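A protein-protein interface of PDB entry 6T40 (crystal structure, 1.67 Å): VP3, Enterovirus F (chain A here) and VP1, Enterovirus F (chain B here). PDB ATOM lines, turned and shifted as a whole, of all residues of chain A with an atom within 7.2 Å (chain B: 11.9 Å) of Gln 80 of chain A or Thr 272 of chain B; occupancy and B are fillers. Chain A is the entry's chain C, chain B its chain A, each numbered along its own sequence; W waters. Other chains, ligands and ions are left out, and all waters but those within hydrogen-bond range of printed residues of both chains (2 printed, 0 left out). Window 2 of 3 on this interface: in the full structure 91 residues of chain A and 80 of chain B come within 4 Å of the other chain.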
ATOM      1  N   ILE A  55       4.929 -24.120   2.786  1.00  0.00           N
ATOM      2  CA  ILE A  55       3.678 -23.465   3.142  1.00  0.00           C
ATOM      3  C   ILE A  55       2.477 -24.313   3.566  1.00  0.00           C
ATOM      4  O   ILE A  55       1.725 -23.911   4.453  1.00  0.00           O
ATOM      5  CB  ILE A  55       3.257 -22.513   1.987  1.00  0.00           C
ATOM      6  CG1 ILE A  55       2.095 -21.623   2.426  1.00  0.00           C
ATOM      7  CG2 ILE A  55       2.919 -23.323   0.742  1.00  0.00           C
ATOM      8  CD1 ILE A  55       2.458 -20.654   3.541  1.00  0.00           C
ATOM      9  N   ASN A  56       2.277 -25.470   2.946  1.00  0.00           N
ATOM     10  CA  ASN A  56       1.139 -26.305   3.315  1.00  0.00           C
ATOM     11  C   ASN A  56       1.570 -27.311   4.376  1.00  0.00           C
ATOM     12  O   ASN A  56       1.515 -28.525   4.168  1.00  0.00           O
ATOM     13  CB  ASN A  56       0.583 -27.017   2.078  1.00  0.00           C
ATOM     14  CG  ASN A  56      -0.794 -27.609   2.319  1.00  0.00           C
ATOM     15  OD1 ASN A  56      -1.576 -27.079   3.109  1.00  0.00           O
ATOM     16  ND2 ASN A  56      -1.102 -28.697   1.627  1.00  0.00           N
ATOM     17  N   VAL A  58       0.496 -28.972   6.964  1.00  0.00           N
ATOM     18  CA  VAL A  58      -0.643 -29.516   7.689  1.00  0.00           C
ATOM     19  C   VAL A  58      -0.544 -31.035   7.727  1.00  0.00           C
ATOM     20  O   VAL A  58       0.162 -31.644   6.923  1.00  0.00           O
ATOM     21  CB  VAL A  58      -1.981 -29.096   7.037  1.00  0.00           C
ATOM     22  CG1 VAL A  58      -2.132 -27.580   7.103  1.00  0.00           C
ATOM     23  CG2 VAL A  58      -2.036 -29.571   5.591  1.00  0.00           C
ATOM     24  N   PRO A  70      -2.979 -25.151  -2.139  1.00  0.00           N
ATOM     25  CA  PRO A  70      -4.160 -25.640  -2.856  1.00  0.00           C
ATOM     26  C   PRO A  70      -5.083 -24.518  -3.319  1.00  0.00           C
ATOM     27  O   PRO A  70      -5.386 -23.593  -2.564  1.00  0.00           O
ATOM     28  CB  PRO A  70      -4.853 -26.536  -1.825  1.00  0.00           C
ATOM     29  CG  PRO A  70      -3.759 -26.888  -0.849  1.00  0.00           C
ATOM     30  CD  PRO A  70      -3.002 -25.598  -0.738  1.00  0.00           C
ATOM     31  N   GLN A  74     -14.225 -22.053  -6.688  1.00  0.00           N
ATOM     32  CA  GLN A  74     -15.087 -21.654  -5.579  1.00  0.00           C
ATOM     33  C   GLN A  74     -16.559 -21.571  -5.962  1.00  0.00           C
ATOM     34  O   GLN A  74     -16.906 -21.509  -7.142  1.00  0.00           O
ATOM     35  CB  GLN A  74     -14.647 -20.283  -5.060  1.00  0.00           C
ATOM     36  CG  GLN A  74     -13.183 -20.208  -4.669  1.00  0.00           C
ATOM     37  CD  GLN A  74     -12.900 -20.957  -3.392  1.00  0.00           C
ATOM     38  OE1 GLN A  74     -13.340 -20.552  -2.317  1.00  0.00           O
ATOM     39  NE2 GLN A  74     -12.172 -22.064  -3.499  1.00  0.00           N
ATOM     40  N   MET A  77     -17.724 -16.123  -2.823  1.00  0.00           N
ATOM     41  CA  MET A  77     -16.736 -15.106  -3.160  1.00  0.00           C
ATOM     42  C   MET A  77     -15.852 -14.623  -2.015  1.00  0.00           C
ATOM     43  O   MET A  77     -16.145 -14.853  -0.842  1.00  0.00           O
ATOM     44  CB  MET A  77     -17.448 -13.910  -3.813  1.00  0.00           C
ATOM     45  CG  MET A  77     -18.062 -14.252  -5.173  1.00  0.00           C
ATOM     46  SD  MET A  77     -19.161 -12.998  -5.873  1.00  0.00           S
ATOM     47  CE  MET A  77     -20.586 -13.116  -4.769  1.00  0.00           C
ATOM     48  N   ASP A  78     -14.744 -13.983  -2.388  1.00  0.00           N
ATOM     49  CA  ASP A  78     -13.787 -13.389  -1.451  1.00  0.00           C
ATOM     50  C   ASP A  78     -13.112 -14.320  -0.437  1.00  0.00           C
ATOM     51  O   ASP A  78     -12.590 -13.849   0.575  1.00  0.00           O
ATOM     52  CB  ASP A  78     -14.471 -12.241  -0.690  1.00  0.00           C
ATOM     53  CG  ASP A  78     -15.425 -11.430  -1.569  1.00  0.00           C
ATOM     54  OD1 ASP A  78     -15.126 -11.225  -2.762  1.00  0.00           O
ATOM     55  OD2 ASP A  78     -16.477 -10.981  -1.061  1.00  0.00           O
ATOM     56  N   GLY A  79     -13.096 -15.623  -0.710  1.00  0.00           N
ATOM     57  CA  GLY A  79     -12.500 -16.576   0.218  1.00  0.00           C
ATOM     58  C   GLY A  79     -10.990 -16.530   0.399  1.00  0.00           C
ATOM     59  O   GLY A  79     -10.260 -16.070  -0.477  1.00  0.00           O
ATOM     60  N   GLN A  80     -10.515 -17.021   1.542  1.00  0.00           N
ATOM     61  CA  GLN A  80      -9.083 -17.030   1.829  1.00  0.00           C
ATOM     62  C   GLN A  80      -8.393 -18.268   1.257  1.00  0.00           C
ATOM     63  O   GLN A  80      -8.988 -19.343   1.176  1.00  0.00           O
ATOM     64  CB  GLN A  80      -8.843 -16.962   3.342  1.00  0.00           C
ATOM     65  CG  GLN A  80      -7.389 -16.687   3.711  1.00  0.00           C
ATOM     66  CD  GLN A  80      -7.180 -16.488   5.201  1.00  0.00           C
ATOM     67  OE1 GLN A  80      -8.106 -16.640   5.999  1.00  0.00           O
ATOM     68  NE2 GLN A  80      -5.954 -16.151   5.585  1.00  0.00           N
ATOM     69  N   ILE A  81      -7.135 -18.106   0.864  1.00  0.00           N
ATOM     70  CA  ILE A  81      -6.349 -19.198   0.296  1.00  0.00           C
ATOM     71  C   ILE A  81      -5.225 -19.624   1.240  1.00  0.00           C
ATOM     72  O   ILE A  81      -4.968 -20.816   1.410  1.00  0.00           O
ATOM     73  CB  ILE A  81      -5.756 -18.783  -1.068  1.00  0.00           C
ATOM     74  CG1 ILE A  81      -6.895 -18.521  -2.057  1.00  0.00           C
ATOM     75  CG2 ILE A  81      -4.820 -19.870  -1.594  1.00  0.00           C
ATOM     76  CD1 ILE A  81      -6.463 -17.826  -3.333  1.00  0.00           C
ATOM     77  N   MET A  82      -4.547 -18.655   1.846  1.00  0.00           N
ATOM     78  CA  MET A  82      -3.472 -18.973   2.782  1.00  0.00           C
ATOM     79  C   MET A  82      -3.089 -17.795   3.663  1.00  0.00           C
ATOM     80  O   MET A  82      -3.524 -16.666   3.436  1.00  0.00           O
ATOM     81  CB  MET A  82      -2.234 -19.503   2.037  1.00  0.00           C
ATOM     82  CG  MET A  82      -1.609 -18.577   1.005  1.00  0.00           C
ATOM     83  SD  MET A  82      -0.788 -17.099   1.670  1.00  0.00           S
ATOM     84  CE  MET A  82       0.313 -17.769   2.767  1.00  0.00           C
ATOM     85  N   ALA A  83      -2.292 -18.080   4.688  1.00  0.00           N
ATOM     86  CA  ALA A  83      -1.818 -17.066   5.622  1.00  0.00           C
ATOM     87  C   ALA A  83      -0.474 -17.518   6.171  1.00  0.00           C
ATOM     88  O   ALA A  83      -0.208 -18.717   6.263  1.00  0.00           O
ATOM     89  CB  ALA A  83      -2.815 -16.886   6.765  1.00  0.00           C
ATOM     90  N   LEU A  84       0.366 -16.559   6.541  1.00  0.00           N
ATOM     91  CA  LEU A  84       1.684 -16.871   7.082  1.00  0.00           C
ATOM     92  C   LEU A  84       2.310 -15.645   7.730  1.00  0.00           C
ATOM     93  O   LEU A  84       2.125 -14.531   7.247  1.00  0.00           O
ATOM     94  CB  LEU A  84       2.608 -17.348   5.954  1.00  0.00           C
ATOM     95  CG  LEU A  84       4.057 -17.681   6.324  1.00  0.00           C
ATOM     96  CD1 LEU A  84       4.092 -18.978   7.104  1.00  0.00           C
ATOM     97  CD2 LEU A  84       4.902 -17.803   5.064  1.00  0.00           C
ATOM     98  N   GLN A 140      -3.910 -11.336  12.336  1.00  0.00           N
ATOM     99  CA  GLN A 140      -3.973 -11.461  10.886  1.00  0.00           C
ATOM    100  C   GLN A 140      -5.366 -11.019  10.439  1.00  0.00           C
ATOM    101  O   GLN A 140      -6.341 -11.191  11.173  1.00  0.00           O
ATOM    102  CB  GLN A 140      -3.722 -12.906  10.450  1.00  0.00           C
ATOM    103  CG  GLN A 140      -4.902 -13.842  10.658  1.00  0.00           C
ATOM    104  CD  GLN A 140      -4.698 -15.179   9.971  1.00  0.00           C
ATOM    105  OE1 GLN A 140      -3.843 -15.965  10.369  1.00  0.00           O
ATOM    106  NE2 GLN A 140      -5.478 -15.437   8.925  1.00  0.00           N
ATOM    107  N   PRO A 141      -5.477 -10.434   9.235  1.00  0.00           N
ATOM    108  CA  PRO A 141      -6.787  -9.987   8.748  1.00  0.00           C
ATOM    109  C   PRO A 141      -7.781 -11.142   8.668  1.00  0.00           C
ATOM    110  O   PRO A 141      -7.428 -12.246   8.258  1.00  0.00           O
ATOM    111  CB  PRO A 141      -6.461  -9.375   7.383  1.00  0.00           C
ATOM    112  CG  PRO A 141      -5.226 -10.116   6.954  1.00  0.00           C
ATOM    113  CD  PRO A 141      -4.428 -10.202   8.228  1.00  0.00           C
ATOM    114  N   THR A 142      -9.022 -10.874   9.066  1.00  0.00           N
ATOM    115  CA  THR A 142     -10.075 -11.886   9.083  1.00  0.00           C
ATOM    116  C   THR A 142     -10.804 -12.072   7.755  1.00  0.00           C
ATOM    117  O   THR A 142     -11.412 -13.115   7.515  1.00  0.00           O
ATOM    118  CB  THR A 142     -11.120 -11.560  10.171  1.00  0.00           C
ATOM    119  OG1 THR A 142     -11.670 -10.257   9.932  1.00  0.00           O
ATOM    120  CG2 THR A 142     -10.475 -11.579  11.549  1.00  0.00           C
ATOM    121  N   ASN A 143     -10.760 -11.060   6.897  1.00  0.00           N
ATOM    122  CA  ASN A 143     -11.416 -11.158   5.600  1.00  0.00           C
ATOM    123  C   ASN A 143     -10.672 -10.343   4.554  1.00  0.00           C
ATOM    124  O   ASN A 143      -9.775  -9.566   4.881  1.00  0.00           O
ATOM    125  CB  ASN A 143     -12.880 -10.708   5.695  1.00  0.00           C
ATOM    126  CG  ASN A 143     -13.032  -9.314   6.268  1.00  0.00           C
ATOM    127  OD1 ASN A 143     -12.430  -8.360   5.782  1.00  0.00           O
ATOM    128  ND2 ASN A 143     -13.848  -9.190   7.308  1.00  0.00           N
ATOM    129  N   ARG A 144     -11.043 -10.527   3.293  1.00  0.00           N
ATOM    130  CA  ARG A 144     -10.383  -9.827   2.198  1.00  0.00           C
ATOM    131  C   ARG A 144     -10.458  -8.307   2.315  1.00  0.00           C
ATOM    132  O   ARG A 144      -9.491  -7.613   1.997  1.00  0.00           O
ATOM    133  CB  ARG A 144     -10.974 -10.268   0.857  1.00  0.00           C
ATOM    134  CG  ARG A 144     -10.135  -9.850  -0.341  1.00  0.00           C
ATOM    135  CD  ARG A 144     -10.768 -10.303  -1.644  1.00  0.00           C
ATOM    136  NE  ARG A 144     -11.915  -9.477  -2.011  1.00  0.00           N
ATOM    137  CZ  ARG A 144     -12.723  -9.739  -3.032  1.00  0.00           C
ATOM    138  NH1 ARG A 144     -12.516 -10.812  -3.785  1.00  0.00           N
ATOM    139  NH2 ARG A 144     -13.725  -8.916  -3.316  1.00  0.00           N
ATOM    140  N   ILE A 195       1.255 -12.257   5.821  1.00  0.00           N
ATOM    141  CA  ILE A 195       1.038 -12.272   4.391  1.00  0.00           C
ATOM    142  C   ILE A 195      -0.166 -13.204   4.242  1.00  0.00           C
ATOM    143  O   ILE A 195      -0.196 -14.288   4.828  1.00  0.00           O
ATOM    144  CB  ILE A 195       2.275 -12.805   3.614  1.00  0.00           C
ATOM    145  CG1 ILE A 195       1.994 -12.769   2.112  1.00  0.00           C
ATOM    146  CG2 ILE A 195       2.624 -14.212   4.066  1.00  0.00           C
ATOM    147  CD1 ILE A 195       3.214 -13.058   1.252  1.00  0.00           C
ATOM    148  N   THR A 196      -1.186 -12.750   3.521  1.00  0.00           N
ATOM    149  CA  THR A 196      -2.381 -13.559   3.305  1.00  0.00           C
ATOM    150  C   THR A 196      -2.756 -13.502   1.832  1.00  0.00           C
ATOM    151  O   THR A 196      -2.433 -12.539   1.139  1.00  0.00           O
ATOM    152  CB  THR A 196      -3.590 -13.068   4.154  1.00  0.00           C
ATOM    153  OG1 THR A 196      -3.874 -11.695   3.855  1.00  0.00           O
ATOM    154  CG2 THR A 196      -3.299 -13.219   5.647  1.00  0.00           C
ATOM    155  N   MET A 197      -3.429 -14.545   1.360  1.00  0.00           N
ATOM    156  CA  MET A 197      -3.844 -14.625  -0.033  1.00  0.00           C
ATOM    157  C   MET A 197      -5.335 -14.919  -0.072  1.00  0.00           C
ATOM    158  O   MET A 197      -5.828 -15.732   0.708  1.00  0.00           O
ATOM    159  CB  MET A 197      -3.074 -15.740  -0.742  1.00  0.00           C
ATOM    160  CG  MET A 197      -3.328 -15.819  -2.238  1.00  0.00           C
ATOM    161  SD  MET A 197      -2.494 -17.241  -2.981  1.00  0.00           S
ATOM    162  CE  MET A 197      -0.793 -16.656  -3.037  1.00  0.00           C
ATOM    163  N   TRP A 198      -6.043 -14.257  -0.984  1.00  0.00           N
ATOM    164  CA  TRP A 198      -7.487 -14.419  -1.118  1.00  0.00           C
ATOM    165  C   TRP A 198      -7.897 -14.479  -2.583  1.00  0.00           C
ATOM    166  O   TRP A 198      -7.179 -14.002  -3.457  1.00  0.00           O
ATOM    167  CB  TRP A 198      -8.219 -13.227  -0.481  1.00  0.00           C
ATOM    168  CG  TRP A 198      -7.693 -12.827   0.862  1.00  0.00           C
ATOM    169  CD1 TRP A 198      -6.504 -12.206   1.129  1.00  0.00           C
ATOM    170  CD2 TRP A 198      -8.306 -13.084   2.127  1.00  0.00           C
ATOM    171  NE1 TRP A 198      -6.337 -12.068   2.487  1.00  0.00           N
ATOM    172  CE2 TRP A 198      -7.429 -12.599   3.123  1.00  0.00           C
ATOM    173  CE3 TRP A 198      -9.514 -13.680   2.519  1.00  0.00           C
ATOM    174  CZ2 TRP A 198      -7.719 -12.695   4.489  1.00  0.00           C
ATOM    175  CZ3 TRP A 198      -9.802 -13.775   3.879  1.00  0.00           C
ATOM    176  CH2 TRP A 198      -8.906 -13.285   4.845  1.00  0.00           C
ATOM    177  N   TYR A 199      -9.055 -15.070  -2.849  1.00  0.00           N
ATOM    178  CA  TYR A 199      -9.560 -15.107  -4.213  1.00  0.00           C
ATOM    179  C   TYR A 199     -10.014 -13.678  -4.505  1.00  0.00           C
ATOM    180  O   TYR A 199     -10.744 -13.088  -3.705  1.00  0.00           O
ATOM    181  CB  TYR A 199     -10.762 -16.056  -4.317  1.00  0.00           C
ATOM    182  CG  TYR A 199     -10.380 -17.516  -4.275  1.00  0.00           C
ATOM    183  CD1 TYR A 199      -9.935 -18.170  -5.425  1.00  0.00           C
ATOM    184  CD2 TYR A 199     -10.398 -18.227  -3.075  1.00  0.00           C
ATOM    185  CE1 TYR A 199      -9.511 -19.500  -5.379  1.00  0.00           C
ATOM    186  CE2 TYR A 199      -9.974 -19.555  -3.017  1.00  0.00           C
ATOM    187  CZ  TYR A 199      -9.530 -20.182  -4.172  1.00  0.00           C
ATOM    188  OH  TYR A 199      -9.084 -21.482  -4.113  1.00  0.00           O
ATOM    189  N   ASN B 267       3.715 -29.164  11.945  1.00  0.00           N
ATOM    190  CA  ASN B 267       2.419 -28.862  11.344  1.00  0.00           C
ATOM    191  C   ASN B 267       1.606 -27.850  12.134  1.00  0.00           C
ATOM    192  O   ASN B 267       1.837 -27.633  13.323  1.00  0.00           O
ATOM    193  CB  ASN B 267       1.575 -30.133  11.206  1.00  0.00           C
ATOM    194  CG  ASN B 267       2.153 -31.113  10.213  1.00  0.00           C
ATOM    195  OD1 ASN B 267       2.697 -30.719   9.183  1.00  0.00           O
ATOM    196  ND2 ASN B 267       2.021 -32.402  10.506  1.00  0.00           N
ATOM    197  N   ARG B 268       0.650 -27.231  11.447  1.00  0.00           N
ATOM    198  CA  ARG B 268      -0.270 -26.283  12.057  1.00  0.00           C
ATOM    199  C   ARG B 268      -1.656 -26.784  11.675  1.00  0.00           C
ATOM    200  O   ARG B 268      -1.789 -27.646  10.804  1.00  0.00           O
ATOM    201  CB  ARG B 268      -0.054 -24.862  11.523  1.00  0.00           C
ATOM    202  CG  ARG B 268      -0.102 -24.733  10.011  1.00  0.00           C
ATOM    203  CD  ARG B 268      -0.148 -23.265   9.603  1.00  0.00           C
ATOM    204  NE  ARG B 268       0.330 -23.058   8.239  1.00  0.00           N
ATOM    205  CZ  ARG B 268       0.151 -21.938   7.544  1.00  0.00           C
ATOM    206  NH1 ARG B 268       0.632 -21.836   6.311  1.00  0.00           N
ATOM    207  NH2 ARG B 268      -0.526 -20.928   8.075  1.00  0.00           N
ATOM    208  N   ALA B 269      -2.686 -26.248  12.320  1.00  0.00           N
ATOM    209  CA  ALA B 269      -4.057 -26.670  12.055  1.00  0.00           C
ATOM    210  C   ALA B 269      -4.497 -26.490  10.606  1.00  0.00           C
ATOM    211  O   ALA B 269      -5.023 -27.419   9.992  1.00  0.00           O
ATOM    212  CB  ALA B 269      -5.015 -25.926  12.983  1.00  0.00           C
ATOM    213  N   ARG B 270      -4.288 -25.299  10.055  1.00  0.00           N
ATOM    214  CA  ARG B 270      -4.705 -25.044   8.682  1.00  0.00           C
ATOM    215  C   ARG B 270      -3.835 -24.004   7.988  1.00  0.00           C
ATOM    216  O   ARG B 270      -3.258 -23.128   8.630  1.00  0.00           O
ATOM    217  CB  ARG B 270      -6.169 -24.601   8.662  1.00  0.00           C
ATOM    218  CG  ARG B 270      -6.434 -23.292   9.378  1.00  0.00           C
ATOM    219  CD  ARG B 270      -7.924 -23.119   9.640  1.00  0.00           C
ATOM    220  NE  ARG B 270      -8.386 -24.016  10.695  1.00  0.00           N
ATOM    221  CZ  ARG B 270      -8.100 -23.858  11.986  1.00  0.00           C
ATOM    222  NH1 ARG B 270      -7.356 -22.833  12.388  1.00  0.00           N
ATOM    223  NH2 ARG B 270      -8.549 -24.733  12.875  1.00  0.00           N
ATOM    224  N   ILE B 271      -3.764 -24.106   6.666  1.00  0.00           N
ATOM    225  CA  ILE B 271      -2.944 -23.209   5.861  1.00  0.00           C
ATOM    226  C   ILE B 271      -3.433 -21.760   5.892  1.00  0.00           C
ATOM    227  O   ILE B 271      -2.677 -20.842   5.568  1.00  0.00           O
ATOM    228  CB  ILE B 271      -2.887 -23.716   4.394  1.00  0.00           C
ATOM    229  CG1 ILE B 271      -1.720 -23.062   3.652  1.00  0.00           C
ATOM    230  CG2 ILE B 271      -4.210 -23.427   3.682  1.00  0.00           C
ATOM    231  CD1 ILE B 271      -1.523 -23.595   2.237  1.00  0.00           C
ATOM    232  N   THR B 272      -4.686 -21.555   6.297  1.00  0.00           N
ATOM    233  CA  THR B 272      -5.273 -20.216   6.350  1.00  0.00           C
ATOM    234  C   THR B 272      -5.160 -19.502   7.695  1.00  0.00           C
ATOM    235  O   THR B 272      -5.672 -18.395   7.855  1.00  0.00           O
ATOM    236  CB  THR B 272      -6.759 -20.251   5.947  1.00  0.00           C
ATOM    237  OG1 THR B 272      -7.431 -21.273   6.693  1.00  0.00           O
ATOM    238  CG2 THR B 272      -6.900 -20.531   4.457  1.00  0.00           C
ATOM    239  N   THR B 273      -4.502 -20.132   8.661  1.00  0.00           N
ATOM    240  CA  THR B 273      -4.318 -19.514   9.972  1.00  0.00           C
ATOM    241  C   THR B 273      -2.827 -19.460  10.274  1.00  0.00           C
ATOM    242  O   THR B 273      -2.187 -20.491  10.479  1.00  0.00           O
ATOM    243  CB  THR B 273      -5.036 -20.305  11.085  1.00  0.00           C
ATOM    244  OG1 THR B 273      -6.446 -20.308  10.829  1.00  0.00           O
ATOM    245  CG2 THR B 273      -4.779 -19.664  12.447  1.00  0.00           C
ATOM    246  N   ALA B 274      -2.282 -18.247  10.285  1.00  0.00           N
ATOM    247  CA  ALA B 274      -0.861 -18.029  10.539  1.00  0.00           C
ATOM    248  C   ALA B 274      -0.487 -18.271  11.997  1.00  0.00           C
ATOM    249  O   ALA B 274       0.654 -18.723  12.238  1.00  0.00           O
ATOM    250  CB  ALA B 274      -0.470 -16.614  10.129  1.00  0.00           C
HETATM  251  O   HOH W   1      -8.405 -17.331   8.680  1.00  0.00           O
HETATM  252  O   HOH W   2       2.070 -34.157   7.758  1.00  0.00           O
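The backbone carbonyl oxygen (O) of Ala 83 of chain A is in hydrogen-bond range of the guanidinium group (NH2) of Arg 268 of chain B, at 2.9 Å. The backbone carbonyl oxygen (O) of Thr 272 of chain B is in hydrogen-bond range of the side-chain amide nitrogen (NE2) of Gln 80 of chain A (3.2 Å). NH1 of Arg 268 of chain B sits at hydrogen-bond distance from O of Ile 55 of chain A (3.0 Å). NE2 of Gln 140 of chain A is in hydrogen-bond range of O of Thr 272 of chain B, 3.2 Å away. The side-chain amide oxygen (OE1) of Gln 140 of chain A is in hydrogen-bond range of the backbone NH (N) of Ala 274 of chain B (2.8 Å). O of Ile 271 of chain B is in hydrogen-bond range of N of Ala 83 of chain A (2.9 Å).
O of Met 197 of chain A lies within hydrogen-bond range of N of Ile 81 of chain A, at 2.7 Å. N of Ile 195 of chain A sits at hydrogen-bond distance from O of Leu 84 of chain A (2.8 Å). N of Met 197 of chain A sits at hydrogen-bond distance from O of Met 82 of chain A, at 3.0 Å. The guanidinium group (NH1) of Arg 270 of chain B sits at hydrogen-bond distance from the side-chain hydroxyl (OG1) of Thr 273 of chain B, at 3.1 Å. The side-chain amide nitrogen of Gln 140 of chain A lies close to the side-chain amide nitrogen of Gln 80 of chain A. The guanidinium group (NH2) of Arg 268 of chain B lies within hydrogen-bond range of the backbone carbonyl oxygen (O) of Thr 273 of chain B.
Ile 55 of chain A touches Ile 271 of chain B. Asn 56 of chain A touches Ile 271 of chain B. Val 58 of chain A touches Asn 267 of chain B (O to OD1, 3.5 Å). Val 58 of chain A touches Arg 268 of chain B (CG1 to O, 3.7 Å). Arg 270 of chain B touches Val 58 of chain A. Ile 271 of chain B touches Val 58 of chain A. Ile 81 of chain A touches Ile 271 of chain B. CA of Met 82 of chain A touches O of Ile 271 of chain B (3.4 Å). Met 82 of chain A touches Thr 272 of chain B. N of Ala 274 of chain B touches CB of Ala 83 of chain A, 3.8 Å away.
Of the printed residues of chain A, Thr 272 of chain B touches Gln 80 (3.2 Å), Ile 81 (3.6 Å), Met 82 (3.98 Å), Ala 83 (3.4 Å) and Gln 140 (3.2 Å). No residue of chain B comes within 4 Å of Gly 79 of chain A. No residue of chain B comes within 4 Å of Thr 196 of chain A. No residue of chain B comes within 4 Å of Tyr 199 of chain A. Printed residues of chain A within 4 Å of Arg 270 of chain B: Val 58 (3.9 Å). Of the printed residues of chain B, Met 82 of chain A touches Ile 271 and Thr 272. Printed residues of chain A within 4 Å of Thr 273 of chain B: Gln 140. Of the printed residues of chain A, Asn 267 of chain B touches Val 58 (3.5 Å). Met 197 of chain A touches none of the printed residues of chain B. Met 77 of chain A touches none of the printed residues of chain B. The nearest printed residue of chain A that does not touch Thr 272 of chain B is Thr 196 of chain A (6.1 Å).
Hydrophobic or aromatic side chains of chain B within 4 Å of the printed part of chain A: Ile 271 and Ala 274. Of the 23 printed residues of chain A, 10 touch a printed residue of chain B. Hydrophobic or aromatic side chains of chain A within 4 Å of the printed part of chain B: Ile 55, Val 58, Pro 70, Met 82 and Ala 83. Among the printed residues, no Asp or Glu carboxylate lies within 4 Å of a Lys or Arg side-chain nitrogen of the other chain.
Water W1 lies within hydrogen-bond range of the side-chain amide oxygen (OE1) of Gln 80 of chain A (2.8 Å), the backbone carbonyl oxygen (O) of Thr 272 of chain B (3.0 Å) and the side-chain amide nitrogen (NE2) of Gln 140 of chain A (3.5 Å). Water W2 lies within hydrogen-bond range of ND2 of Asn 267 of chain B (3.3 Å) and O of Val 58 of chain A (3.3 Å).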
